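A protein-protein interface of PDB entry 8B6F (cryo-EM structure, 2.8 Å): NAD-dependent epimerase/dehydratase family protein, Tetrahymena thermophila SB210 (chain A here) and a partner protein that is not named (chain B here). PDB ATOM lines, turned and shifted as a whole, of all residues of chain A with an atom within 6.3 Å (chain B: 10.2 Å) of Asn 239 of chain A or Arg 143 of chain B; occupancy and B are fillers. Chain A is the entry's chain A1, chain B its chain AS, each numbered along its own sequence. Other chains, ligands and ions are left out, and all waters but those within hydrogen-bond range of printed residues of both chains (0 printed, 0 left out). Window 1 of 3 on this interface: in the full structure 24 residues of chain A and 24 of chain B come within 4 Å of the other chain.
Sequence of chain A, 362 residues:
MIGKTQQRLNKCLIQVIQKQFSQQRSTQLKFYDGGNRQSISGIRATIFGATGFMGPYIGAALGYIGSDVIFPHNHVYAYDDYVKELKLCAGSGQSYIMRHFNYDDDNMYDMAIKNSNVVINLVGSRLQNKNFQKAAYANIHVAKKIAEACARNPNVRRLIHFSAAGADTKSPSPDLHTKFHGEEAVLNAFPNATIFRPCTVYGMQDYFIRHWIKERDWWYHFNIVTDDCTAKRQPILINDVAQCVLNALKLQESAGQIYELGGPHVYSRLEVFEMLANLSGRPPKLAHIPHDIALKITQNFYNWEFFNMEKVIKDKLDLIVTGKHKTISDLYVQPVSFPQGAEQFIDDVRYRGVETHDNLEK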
ATOM      1  N   TYR A  57      -1.377  -7.720 -26.345  1.00  0.00           N
ATOM      2  CA  TYR A  57      -0.676  -7.231 -25.162  1.00  0.00           C
ATOM      3  C   TYR A  57      -0.598  -8.303 -24.082  1.00  0.00           C
ATOM      4  O   TYR A  57       0.466  -8.529 -23.494  1.00  0.00           O
ATOM      5  CB  TYR A  57      -1.373  -5.979 -24.629  1.00  0.00           C
ATOM      6  CG  TYR A  57      -1.168  -4.757 -25.486  1.00  0.00           C
ATOM      7  CD1 TYR A  57      -1.976  -4.509 -26.587  1.00  0.00           C
ATOM      8  CD2 TYR A  57      -0.166  -3.844 -25.190  1.00  0.00           C
ATOM      9  CE1 TYR A  57      -1.791  -3.389 -27.370  1.00  0.00           C
ATOM     10  CE2 TYR A  57       0.027  -2.722 -25.965  1.00  0.00           C
ATOM     11  CZ  TYR A  57      -0.788  -2.498 -27.053  1.00  0.00           C
ATOM     12  OH  TYR A  57      -0.595  -1.380 -27.827  1.00  0.00           O
ATOM     13  N   VAL A 201     -10.509   0.204 -20.890  1.00  0.00           N
ATOM     14  CA  VAL A 201      -9.071   0.171 -21.125  1.00  0.00           C
ATOM     15  C   VAL A 201      -8.749   1.010 -22.352  1.00  0.00           C
ATOM     16  O   VAL A 201      -9.445   0.939 -23.372  1.00  0.00           O
ATOM     17  CB  VAL A 201      -8.584  -1.279 -21.299  1.00  0.00           C
ATOM     18  CG1 VAL A 201      -7.069  -1.322 -21.418  1.00  0.00           C
ATOM     19  CG2 VAL A 201      -9.057  -2.145 -20.144  1.00  0.00           C
ATOM     20  N   TYR A 202      -7.690   1.809 -22.261  1.00  0.00           N
ATOM     21  CA  TYR A 202      -7.277   2.678 -23.351  1.00  0.00           C
ATOM     22  C   TYR A 202      -5.837   2.375 -23.746  1.00  0.00           C
ATOM     23  O   TYR A 202      -5.044   1.853 -22.957  1.00  0.00           O
ATOM     24  CB  TYR A 202      -7.427   4.157 -22.977  1.00  0.00           C
ATOM     25  CG  TYR A 202      -6.531   4.609 -21.855  1.00  0.00           C
ATOM     26  CD1 TYR A 202      -6.926   4.474 -20.533  1.00  0.00           C
ATOM     27  CD2 TYR A 202      -5.297   5.185 -22.116  1.00  0.00           C
ATOM     28  CE1 TYR A 202      -6.116   4.889 -19.503  1.00  0.00           C
ATOM     29  CE2 TYR A 202      -4.477   5.605 -21.091  1.00  0.00           C
ATOM     30  CZ  TYR A 202      -4.895   5.453 -19.787  1.00  0.00           C
ATOM     31  OH  TYR A 202      -4.091   5.865 -18.755  1.00  0.00           O
ATOM     32  N   LEU A 237      -4.847   1.805 -18.013  1.00  0.00           N
ATOM     33  CA  LEU A 237      -3.932   1.553 -19.117  1.00  0.00           C
ATOM     34  C   LEU A 237      -3.774   0.058 -19.356  1.00  0.00           C
ATOM     35  O   LEU A 237      -3.777  -0.742 -18.416  1.00  0.00           O
ATOM     36  CB  LEU A 237      -2.570   2.183 -18.830  1.00  0.00           C
ATOM     37  CG  LEU A 237      -1.549   2.154 -19.968  1.00  0.00           C
ATOM     38  CD1 LEU A 237      -2.035   2.945 -21.167  1.00  0.00           C
ATOM     39  CD2 LEU A 237      -0.210   2.682 -19.484  1.00  0.00           C
ATOM     40  N   ILE A 238      -3.626  -0.316 -20.627  1.00  0.00           N
ATOM     41  CA  ILE A 238      -3.485  -1.724 -20.979  1.00  0.00           C
ATOM     42  C   ILE A 238      -2.194  -2.301 -20.417  1.00  0.00           C
ATOM     43  O   ILE A 238      -2.144  -3.480 -20.047  1.00  0.00           O
ATOM     44  CB  ILE A 238      -3.571  -1.909 -22.503  1.00  0.00           C
ATOM     45  CG1 ILE A 238      -3.593  -3.398 -22.838  1.00  0.00           C
ATOM     46  CG2 ILE A 238      -2.406  -1.218 -23.198  1.00  0.00           C
ATOM     47  CD1 ILE A 238      -4.108  -3.695 -24.203  1.00  0.00           C
ATOM     48  N   ASN A 239      -1.131  -1.499 -20.351  1.00  0.00           N
ATOM     49  CA  ASN A 239       0.084  -1.951 -19.684  1.00  0.00           C
ATOM     50  C   ASN A 239      -0.190  -2.286 -18.225  1.00  0.00           C
ATOM     51  O   ASN A 239       0.316  -3.286 -17.703  1.00  0.00           O
ATOM     52  CB  ASN A 239       1.170  -0.881 -19.793  1.00  0.00           C
ATOM     53  CG  ASN A 239       1.454  -0.485 -21.226  1.00  0.00           C
ATOM     54  OD1 ASN A 239       0.659  -0.753 -22.123  1.00  0.00           O
ATOM     55  ND2 ASN A 239       2.593   0.158 -21.448  1.00  0.00           N
ATOM     56  N   ASP A 240      -0.991  -1.462 -17.549  1.00  0.00           N
ATOM     57  CA  ASP A 240      -1.367  -1.764 -16.172  1.00  0.00           C
ATOM     58  C   ASP A 240      -2.170  -3.056 -16.090  1.00  0.00           C
ATOM     59  O   ASP A 240      -2.005  -3.839 -15.148  1.00  0.00           O
ATOM     60  CB  ASP A 240      -2.163  -0.600 -15.584  1.00  0.00           C
ATOM     61  CG  ASP A 240      -1.398   0.704 -15.625  1.00  0.00           C
ATOM     62  OD1 ASP A 240      -0.151   0.662 -15.681  1.00  0.00           O
ATOM     63  OD2 ASP A 240      -2.041   1.774 -15.605  1.00  0.00           O
ATOM     64  N   VAL A 241      -3.057  -3.293 -17.058  1.00  0.00           N
ATOM     65  CA  VAL A 241      -3.832  -4.532 -17.065  1.00  0.00           C
ATOM     66  C   VAL A 241      -2.907  -5.734 -17.215  1.00  0.00           C
ATOM     67  O   VAL A 241      -3.076  -6.754 -16.538  1.00  0.00           O
ATOM     68  CB  VAL A 241      -4.895  -4.494 -18.178  1.00  0.00           C
ATOM     69  CG1 VAL A 241      -5.648  -5.817 -18.250  1.00  0.00           C
ATOM     70  CG2 VAL A 241      -5.860  -3.347 -17.951  1.00  0.00           C
ATOM     71  N   ALA A 242      -1.920  -5.637 -18.110  1.00  0.00           N
ATOM     72  CA  ALA A 242      -0.975  -6.734 -18.287  1.00  0.00           C
ATOM     73  C   ALA A 242      -0.168  -6.973 -17.019  1.00  0.00           C
ATOM     74  O   ALA A 242       0.057  -8.121 -16.622  1.00  0.00           O
ATOM     75  CB  ALA A 242      -0.046  -6.439 -19.464  1.00  0.00           C
ATOM     76  N   GLN A 243       0.278  -5.897 -16.369  1.00  0.00           N
ATOM     77  CA  GLN A 243       1.002  -6.040 -15.111  1.00  0.00           C
ATOM     78  C   GLN A 243       0.119  -6.676 -14.048  1.00  0.00           C
ATOM     79  O   GLN A 243       0.592  -7.473 -13.229  1.00  0.00           O
ATOM     80  CB  GLN A 243       1.518  -4.680 -14.645  1.00  0.00           C
ATOM     81  CG  GLN A 243       2.495  -4.760 -13.485  1.00  0.00           C
ATOM     82  CD  GLN A 243       3.761  -5.511 -13.841  1.00  0.00           C
ATOM     83  OE1 GLN A 243       4.727  -4.928 -14.329  1.00  0.00           O
ATOM     84  NE2 GLN A 243       3.760  -6.816 -13.599  1.00  0.00           N
ATOM     85  N   CYS A 244      -1.170  -6.334 -14.043  1.00  0.00           N
ATOM     86  CA  CYS A 244      -2.102  -6.966 -13.118  1.00  0.00           C
ATOM     87  C   CYS A 244      -2.219  -8.461 -13.386  1.00  0.00           C
ATOM     88  O   CYS A 244      -2.285  -9.263 -12.447  1.00  0.00           O
ATOM     89  CB  CYS A 244      -3.474  -6.302 -13.231  1.00  0.00           C
ATOM     90  SG  CYS A 244      -3.566  -4.666 -12.488  1.00  0.00           S
ATOM     91  N   VAL A 333      -0.658  -3.300  -7.951  1.00  0.00           N
ATOM     92  CA  VAL A 333      -0.302  -2.546  -9.146  1.00  0.00           C
ATOM     93  C   VAL A 333      -0.800  -1.120  -8.972  1.00  0.00           C
ATOM     94  O   VAL A 333      -1.970  -0.902  -8.636  1.00  0.00           O
ATOM     95  CB  VAL A 333      -0.891  -3.184 -10.416  1.00  0.00           C
ATOM     96  CG1 VAL A 333      -0.565  -2.342 -11.642  1.00  0.00           C
ATOM     97  CG2 VAL A 333      -0.368  -4.594 -10.590  1.00  0.00           C
ATOM     98  N   GLN A 334       0.088  -0.150  -9.193  1.00  0.00           N
ATOM     99  CA  GLN A 334      -0.259   1.259  -9.081  1.00  0.00           C
ATOM    100  C   GLN A 334      -0.571   1.803 -10.470  1.00  0.00           C
ATOM    101  O   GLN A 334       0.358   2.161 -11.208  1.00  0.00           O
ATOM    102  CB  GLN A 334       0.886   2.044  -8.438  1.00  0.00           C
ATOM    103  CG  GLN A 334       0.616   3.533  -8.299  1.00  0.00           C
ATOM    104  CD  GLN A 334      -0.638   3.828  -7.504  1.00  0.00           C
ATOM    105  OE1 GLN A 334      -1.465   4.643  -7.909  1.00  0.00           O
ATOM    106  NE2 GLN A 334      -0.782   3.171  -6.359  1.00  0.00           N
ATOM    107  N   PRO A 335      -1.835   1.887 -10.877  1.00  0.00           N
ATOM    108  CA  PRO A 335      -2.135   2.395 -12.220  1.00  0.00           C
ATOM    109  C   PRO A 335      -1.768   3.862 -12.362  1.00  0.00           C
ATOM    110  O   PRO A 335      -1.801   4.634 -11.401  1.00  0.00           O
ATOM    111  CB  PRO A 335      -3.647   2.185 -12.349  1.00  0.00           C
ATOM    112  CG  PRO A 335      -4.143   2.212 -10.953  1.00  0.00           C
ATOM    113  CD  PRO A 335      -3.061   1.600 -10.113  1.00  0.00           C
ATOM    114  N   VAL A 336      -1.420   4.243 -13.583  1.00  0.00           N
ATOM    115  CA  VAL A 336      -1.055   5.624 -13.872  1.00  0.00           C
ATOM    116  C   VAL A 336      -2.317   6.428 -14.144  1.00  0.00           C
ATOM    117  O   VAL A 336      -3.326   5.906 -14.632  1.00  0.00           O
ATOM    118  CB  VAL A 336      -0.069   5.694 -15.054  1.00  0.00           C
ATOM    119  CG1 VAL A 336      -0.747   5.278 -16.352  1.00  0.00           C
ATOM    120  CG2 VAL A 336       0.526   7.091 -15.174  1.00  0.00           C
ATOM    121  N   GLN A 340      -1.857  11.485 -17.625  1.00  0.00           N
ATOM    122  CA  GLN A 340      -0.476  11.135 -17.940  1.00  0.00           C
ATOM    123  C   GLN A 340      -0.409   9.987 -18.936  1.00  0.00           C
ATOM    124  O   GLN A 340       0.399  10.014 -19.871  1.00  0.00           O
ATOM    125  CB  GLN A 340       0.272  10.768 -16.659  1.00  0.00           C
ATOM    126  CG  GLN A 340       1.771  10.603 -16.838  1.00  0.00           C
ATOM    127  CD  GLN A 340       2.491  11.923 -16.983  1.00  0.00           C
ATOM    128  OE1 GLN A 340       1.881  12.987 -16.908  1.00  0.00           O
ATOM    129  NE2 GLN A 340       3.800  11.861 -17.186  1.00  0.00           N
ATOM    130  N   GLN A 344       0.607  10.386 -24.500  1.00  0.00           N
ATOM    131  CA  GLN A 344       1.507   9.928 -25.554  1.00  0.00           C
ATOM    132  C   GLN A 344       0.750   9.452 -26.788  1.00  0.00           C
ATOM    133  O   GLN A 344       1.291   9.494 -27.897  1.00  0.00           O
ATOM    134  CB  GLN A 344       2.406   8.809 -25.031  1.00  0.00           C
ATOM    135  CG  GLN A 344       1.652   7.568 -24.584  1.00  0.00           C
ATOM    136  CD  GLN A 344       2.578   6.447 -24.155  1.00  0.00           C
ATOM    137  OE1 GLN A 344       3.755   6.425 -24.512  1.00  0.00           O
ATOM    138  NE2 GLN A 344       2.049   5.509 -23.377  1.00  0.00           N
ATOM    139  N   PHE A 345      -0.489   8.995 -26.621  1.00  0.00           N
ATOM    140  CA  PHE A 345      -1.243   8.420 -27.727  1.00  0.00           C
ATOM    141  C   PHE A 345      -1.942   9.465 -28.584  1.00  0.00           C
ATOM    142  O   PHE A 345      -2.611   9.096 -29.554  1.00  0.00           O
ATOM    143  CB  PHE A 345      -2.273   7.424 -27.189  1.00  0.00           C
ATOM    144  CG  PHE A 345      -1.674   6.336 -26.351  1.00  0.00           C
ATOM    145  CD1 PHE A 345      -0.998   5.283 -26.941  1.00  0.00           C
ATOM    146  CD2 PHE A 345      -1.785   6.365 -24.972  1.00  0.00           C
ATOM    147  CE1 PHE A 345      -0.443   4.280 -26.173  1.00  0.00           C
ATOM    148  CE2 PHE A 345      -1.233   5.365 -24.196  1.00  0.00           C
ATOM    149  CZ  PHE A 345      -0.561   4.321 -24.797  1.00  0.00           C
ATOM    150  N   GLY B  77       8.373  13.005 -23.630  1.00  0.00           N
ATOM    151  CA  GLY B  77       8.180  13.883 -22.489  1.00  0.00           C
ATOM    152  C   GLY B  77       7.353  13.250 -21.389  1.00  0.00           C
ATOM    153  O   GLY B  77       7.587  13.506 -20.206  1.00  0.00           O
ATOM    154  N   THR B  78       6.371  12.426 -21.760  1.00  0.00           N
ATOM    155  CA  THR B  78       5.528  11.780 -20.759  1.00  0.00           C
ATOM    156  C   THR B  78       6.333  10.816 -19.895  1.00  0.00           C
ATOM    157  O   THR B  78       6.101  10.714 -18.686  1.00  0.00           O
ATOM    158  CB  THR B  78       4.378  11.043 -21.445  1.00  0.00           C
ATOM    159  OG1 THR B  78       3.697  11.938 -22.333  1.00  0.00           O
ATOM    160  CG2 THR B  78       3.389  10.513 -20.418  1.00  0.00           C
ATOM    161  N   LYS B  79       7.280  10.096 -20.499  1.00  0.00           N
ATOM    162  CA  LYS B  79       8.044   9.103 -19.750  1.00  0.00           C
ATOM    163  C   LYS B  79       8.818   9.746 -18.609  1.00  0.00           C
ATOM    164  O   LYS B  79       8.911   9.179 -17.514  1.00  0.00           O
ATOM    165  CB  LYS B  79       8.993   8.358 -20.687  1.00  0.00           C
ATOM    166  CG  LYS B  79       8.290   7.431 -21.666  1.00  0.00           C
ATOM    167  CD  LYS B  79       9.271   6.813 -22.648  1.00  0.00           C
ATOM    168  CE  LYS B  79       8.576   5.836 -23.583  1.00  0.00           C
ATOM    169  NZ  LYS B  79       7.510   6.494 -24.392  1.00  0.00           N
ATOM    170  N   PHE B  80       9.389  10.923 -18.843  1.00  0.00           N
ATOM    171  CA  PHE B  80      10.143  11.620 -17.811  1.00  0.00           C
ATOM    172  C   PHE B  80      10.146  13.108 -18.119  1.00  0.00           C
ATOM    173  O   PHE B  80      10.096  13.516 -19.281  1.00  0.00           O
ATOM    174  CB  PHE B  80      11.577  11.088 -17.714  1.00  0.00           C
ATOM    175  CG  PHE B  80      12.094  10.508 -19.000  1.00  0.00           C
ATOM    176  CD1 PHE B  80      12.316  11.317 -20.099  1.00  0.00           C
ATOM    177  CD2 PHE B  80      12.368   9.156 -19.102  1.00  0.00           C
ATOM    178  CE1 PHE B  80      12.791  10.786 -21.280  1.00  0.00           C
ATOM    179  CE2 PHE B  80      12.844   8.619 -20.280  1.00  0.00           C
ATOM    180  CZ  PHE B  80      13.056   9.435 -21.371  1.00  0.00           C
ATOM    181  N   HIS B 126      13.666   6.576 -30.345  1.00  0.00           N
ATOM    182  CA  HIS B 126      13.397   7.046 -28.990  1.00  0.00           C
ATOM    183  C   HIS B 126      13.530   5.912 -27.980  1.00  0.00           C
ATOM    184  O   HIS B 126      14.099   6.100 -26.899  1.00  0.00           O
ATOM    185  CB  HIS B 126      12.014   7.699 -28.915  1.00  0.00           C
ATOM    186  CG  HIS B 126      10.873   6.748 -29.095  1.00  0.00           C
ATOM    187  ND1 HIS B 126      10.511   6.242 -30.325  1.00  0.00           N
ATOM    188  CD2 HIS B 126       9.988   6.241 -28.205  1.00  0.00           C
ATOM    189  CE1 HIS B 126       9.465   5.447 -30.181  1.00  0.00           C
ATOM    190  NE2 HIS B 126       9.125   5.433 -28.905  1.00  0.00           N
ATOM    191  N   THR B 127      13.005   4.729 -28.307  1.00  0.00           N
ATOM    192  CA  THR B 127      13.100   3.603 -27.384  1.00  0.00           C
ATOM    193  C   THR B 127      14.539   3.134 -27.208  1.00  0.00           C
ATOM    194  O   THR B 127      14.891   2.612 -26.144  1.00  0.00           O
ATOM    195  CB  THR B 127      12.236   2.439 -27.868  1.00  0.00           C
ATOM    196  OG1 THR B 127      12.670   2.019 -29.168  1.00  0.00           O
ATOM    197  CG2 THR B 127      10.781   2.844 -27.933  1.00  0.00           C
ATOM    198  N   MET B 130      16.396   6.213 -25.075  1.00  0.00           N
ATOM    199  CA  MET B 130      15.901   6.559 -23.750  1.00  0.00           C
ATOM    200  C   MET B 130      16.548   5.730 -22.651  1.00  0.00           C
ATOM    201  O   MET B 130      16.305   6.007 -21.471  1.00  0.00           O
ATOM    202  CB  MET B 130      14.382   6.390 -23.690  1.00  0.00           C
ATOM    203  CG  MET B 130      13.905   4.951 -23.805  1.00  0.00           C
ATOM    204  SD  MET B 130      12.110   4.831 -23.727  1.00  0.00           S
ATOM    205  CE  MET B 130      11.896   3.056 -23.695  1.00  0.00           C
ATOM    206  N   SER B 134      16.608   6.994 -18.769  1.00  0.00           N
ATOM    207  CA  SER B 134      15.678   6.293 -17.901  1.00  0.00           C
ATOM    208  C   SER B 134      16.128   6.374 -16.442  1.00  0.00           C
ATOM    209  O   SER B 134      17.327   6.389 -16.155  1.00  0.00           O
ATOM    210  CB  SER B 134      15.561   4.830 -18.317  1.00  0.00           C
ATOM    211  OG  SER B 134      15.117   4.714 -19.657  1.00  0.00           O
ATOM    212  N   PRO B 135      15.186   6.421 -15.498  1.00  0.00           N
ATOM    213  CA  PRO B 135      15.573   6.440 -14.083  1.00  0.00           C
ATOM    214  C   PRO B 135      16.272   5.152 -13.676  1.00  0.00           C
ATOM    215  O   PRO B 135      15.986   4.072 -14.195  1.00  0.00           O
ATOM    216  CB  PRO B 135      14.238   6.604 -13.346  1.00  0.00           C
ATOM    217  CG  PRO B 135      13.286   7.112 -14.363  1.00  0.00           C
ATOM    218  CD  PRO B 135      13.726   6.530 -15.662  1.00  0.00           C
ATOM    219  N   THR B 138      13.650   4.507 -10.216  1.00  0.00           N
ATOM    220  CA  THR B 138      12.311   5.062 -10.147  1.00  0.00           C
ATOM    221  C   THR B 138      11.468   4.566 -11.319  1.00  0.00           C
ATOM    222  O   THR B 138      11.994   4.352 -12.416  1.00  0.00           O
ATOM    223  CB  THR B 138      12.358   6.596 -10.170  1.00  0.00           C
ATOM    224  OG1 THR B 138      13.221   7.067  -9.126  1.00  0.00           O
ATOM    225  CG2 THR B 138      10.970   7.192  -9.984  1.00  0.00           C
ATOM    226  N   PRO B 139      10.167   4.360 -11.127  1.00  0.00           N
ATOM    227  CA  PRO B 139       9.328   3.923 -12.247  1.00  0.00           C
ATOM    228  C   PRO B 139       9.233   4.975 -13.338  1.00  0.00           C
ATOM    229  O   PRO B 139       9.344   6.178 -13.092  1.00  0.00           O
ATOM    230  CB  PRO B 139       7.961   3.684 -11.597  1.00  0.00           C
ATOM    231  CG  PRO B 139       8.242   3.496 -10.161  1.00  0.00           C
ATOM    232  CD  PRO B 139       9.417   4.364  -9.860  1.00  0.00           C
ATOM    233  N   LEU B 140       9.030   4.501 -14.563  1.00  0.00           N
ATOM    234  CA  LEU B 140       8.769   5.398 -15.678  1.00  0.00           C
ATOM    235  C   LEU B 140       7.424   6.087 -15.480  1.00  0.00           C
ATOM    236  O   LEU B 140       6.455   5.470 -15.031  1.00  0.00           O
ATOM    237  CB  LEU B 140       8.788   4.622 -16.995  1.00  0.00           C
ATOM    238  CG  LEU B 140       9.400   5.319 -18.215  1.00  0.00           C
ATOM    239  CD1 LEU B 140      10.865   5.666 -17.980  1.00  0.00           C
ATOM    240  CD2 LEU B 140       9.259   4.447 -19.450  1.00  0.00           C
ATOM    241  N   SER B 141       7.366   7.376 -15.819  1.00  0.00           N
ATOM    242  CA  SER B 141       6.205   8.191 -15.480  1.00  0.00           C
ATOM    243  C   SER B 141       4.988   7.909 -16.350  1.00  0.00           C
ATOM    244  O   SER B 141       3.897   8.385 -16.021  1.00  0.00           O
ATOM    245  CB  SER B 141       6.561   9.676 -15.585  1.00  0.00           C
ATOM    246  OG  SER B 141       7.631  10.010 -14.717  1.00  0.00           O
ATOM    247  N   ASP B 142       5.135   7.161 -17.440  1.00  0.00           N
ATOM    248  CA  ASP B 142       4.029   6.883 -18.348  1.00  0.00           C
ATOM    249  C   ASP B 142       3.425   5.502 -18.134  1.00  0.00           C
ATOM    250  O   ASP B 142       2.595   5.071 -18.941  1.00  0.00           O
ATOM    251  CB  ASP B 142       4.493   7.024 -19.798  1.00  0.00           C
ATOM    252  CG  ASP B 142       5.551   6.011 -20.168  1.00  0.00           C
ATOM    253  OD1 ASP B 142       6.374   5.670 -19.294  1.00  0.00           O
ATOM    254  OD2 ASP B 142       5.563   5.555 -21.331  1.00  0.00           O
ATOM    255  N   ARG B 143       3.816   4.802 -17.074  1.00  0.00           N
ATOM    256  CA  ARG B 143       3.366   3.443 -16.824  1.00  0.00           C
ATOM    257  C   ARG B 143       2.972   3.291 -15.364  1.00  0.00           C
ATOM    258  O   ARG B 143       3.443   4.024 -14.491  1.00  0.00           O
ATOM    259  CB  ARG B 143       4.457   2.417 -17.162  1.00  0.00           C
ATOM    260  CG  ARG B 143       4.879   2.398 -18.617  1.00  0.00           C
ATOM    261  CD  ARG B 143       6.182   1.636 -18.785  1.00  0.00           C
ATOM    262  NE  ARG B 143       6.491   1.374 -20.185  1.00  0.00           N
ATOM    263  CZ  ARG B 143       6.088   0.305 -20.857  1.00  0.00           C
ATOM    264  NH1 ARG B 143       5.342  -0.631 -20.289  1.00  0.00           N
ATOM    265  NH2 ARG B 143       6.440   0.168 -22.132  1.00  0.00           N
ATOM    266  N   GLY B 144       2.094   2.329 -15.110  1.00  0.00           N
ATOM    267  CA  GLY B 144       1.767   1.954 -13.752  1.00  0.00           C
ATOM    268  C   GLY B 144       2.727   0.903 -13.238  1.00  0.00           C
ATOM    269  O   GLY B 144       2.893  -0.148 -13.862  1.00  0.00           O
ATOM    270  N   TYR B 145       3.368   1.174 -12.109  1.00  0.00           N
ATOM    271  CA  TYR B 145       4.385   0.279 -11.582  1.00  0.00           C
ATOM    272  C   TYR B 145       3.773  -0.750 -10.641  1.00  0.00           C
ATOM    273  O   TYR B 145       2.667  -0.583 -10.123  1.00  0.00           O
ATOM    274  CB  TYR B 145       5.477   1.068 -10.860  1.00  0.00           C
ATOM    275  CG  TYR B 145       4.978   1.917  -9.716  1.00  0.00           C
ATOM    276  CD1 TYR B 145       4.859   1.397  -8.437  1.00  0.00           C
ATOM    277  CD2 TYR B 145       4.643   3.247  -9.916  1.00  0.00           C
ATOM    278  CE1 TYR B 145       4.409   2.175  -7.391  1.00  0.00           C
ATOM    279  CE2 TYR B 145       4.194   4.033  -8.878  1.00  0.00           C
ATOM    280  CZ  TYR B 145       4.080   3.492  -7.618  1.00  0.00           C
ATOM    281  OH  TYR B 145       3.631   4.274  -6.581  1.00  0.00           O
ATOM    282  N   SER B 146       4.519  -1.827 -10.425  1.00  0.00           N
ATOM    283  CA  SER B 146       4.118  -2.914  -9.544  1.00  0.00           C
ATOM    284  C   SER B 146       5.019  -2.904  -8.319  1.00  0.00           C
ATOM    285  O   SER B 146       6.243  -3.024  -8.444  1.00  0.00           O
ATOM    286  CB  SER B 146       4.210  -4.258 -10.267  1.00  0.00           C
ATOM    287  OG  SER B 146       4.046  -5.337  -9.365  1.00  0.00           O
ATOM    288  N   TYR B 147       4.414  -2.763  -7.140  1.00  0.00           N
ATOM    289  CA  TYR B 147       5.135  -2.810  -5.874  1.00  0.00           C
ATOM    290  C   TYR B 147       4.900  -4.126  -5.140  1.00  0.00           C
ATOM    291  O   TYR B 147       5.062  -4.191  -3.918  1.00  0.00           O
ATOM    292  CB  TYR B 147       4.743  -1.625  -4.989  1.00  0.00           C
ATOM    293  CG  TYR B 147       3.254  -1.446  -4.811  1.00  0.00           C
ATOM    294  CD1 TYR B 147       2.516  -0.669  -5.692  1.00  0.00           C
ATOM    295  CD2 TYR B 147       2.588  -2.048  -3.755  1.00  0.00           C
ATOM    296  CE1 TYR B 147       1.156  -0.502  -5.530  1.00  0.00           C
ATOM    297  CE2 TYR B 147       1.228  -1.888  -3.583  1.00  0.00           C
ATOM    298  CZ  TYR B 147       0.518  -1.114  -4.474  1.00  0.00           C
ATOM    299  OH  TYR B 147      -0.836  -0.953  -4.306  1.00  0.00           O
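The side-chain amide nitrogen (ND2) of Asn 239 of chain A lies close to the guanidinium group (NH1) of Arg 143 of chain B (3.1 Å).
OD1 of Asp 240 of chain A lies within hydrogen-bond range of N of Gly 144 of chain B, 2.9 Å away.
The backbone NH (N) of Gln 334 of chain A is in hydrogen-bond range of the backbone carbonyl oxygen (O) of Tyr 145 of chain B (2.8 Å).
The backbone carbonyl oxygen (O) of Thr 78 of chain B sits at hydrogen-bond distance from the side-chain amide nitrogen (NE2) of Gln 340 of chain A (3.0 Å).
The backbone carbonyl oxygen (O) of Asp 240 of chain A lies within hydrogen-bond range of the side-chain sulfur (SG) of Cys 244 of chain A (3.2 Å).
N of Val 336 of chain A lies within hydrogen-bond range of OD2 of Asp 240 of chain A (3.3 Å).
O of Lys 79 of chain B is in hydrogen-bond range of N of Ser 141 of chain B (2.9 Å).
The side-chain carboxylate (OD2) of Asp 142 of chain B lies within salt-bridge range of the side-chain amino group (NZ) of Lys 79 of chain B (3.7 Å).
Among the printed residues, pairs that only touch across the chains: Gln 334 of chain A with Gly 144 of chain B (2.9 Å), Gln 340 of chain A with Ser 141 of chain B (3.2 Å), Gln 243 of chain A with Ser 146 of chain B (3.7 Å), Val 333 of chain A with Tyr 145 of chain B (3.7 Å), Val 336 of chain A with Ser 141 of chain B (3.7 Å), Leu 237 of chain A with Asp 142 of chain B (3.7 Å), Gln 344 of chain A with Lys 79 of chain B (3.8 Å), Gln 344 of chain A with Asp 142 of chain B (3.8 Å), Gln 334 of chain A with Tyr 147 of chain B (3.8 Å), Val 336 of chain A with Arg 143 of chain B (3.9 Å) and Val 336 of chain A with Gly 144 of chain B (3.9 Å).
Hydrophobic or aromatic side chains of chain A that line the printed part of chain B: Leu 237, Val 333 and Val 336.
Hydrophobic or aromatic side chains of chain B within 4 Å of the printed part of chain A: Tyr 145 and Tyr 147.
Among the printed residues, 15 pairs touch across the chains.
Among the printed residues, no Asp or Glu carboxylate lies within 4 Å of a Lys or Arg side-chain nitrogen of the other chain.
Asn 239 of chain A touches just one residue of chain B: Arg 143 (3.1 Å).
Of chain A, only Asn 239 (3.1 Å) and Val 336 (3.9 Å) come within 4 Å of Arg 143 of chain B.
No residue of chain B comes within 4 Å of Ile 238 of chain A.
Of chain B, only Gly 144 comes within 4 Å of Asp 240 of chain A.
No residue of chain B comes within 4 Å of Ala 242 of chain A.
Of the printed residues of chain A, Asp 142 of chain B touches Leu 237 (3.7 Å) and Gln 344 (3.8 Å).
Printed residues of chain B within 4 Å of Gln 344 of chain A: Lys 79 (3.8 Å) and Asp 142 (3.8 Å).
Tyr 202 of chain A touches none of the printed residues of chain B.
The nearest residue of chain B that does not touch Asn 239 of chain A is Asp 142 of chain B (5.5 Å).
The nearest residue of chain A that does not touch Arg 143 of chain B is Asp 240 of chain A (4.1 Å).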
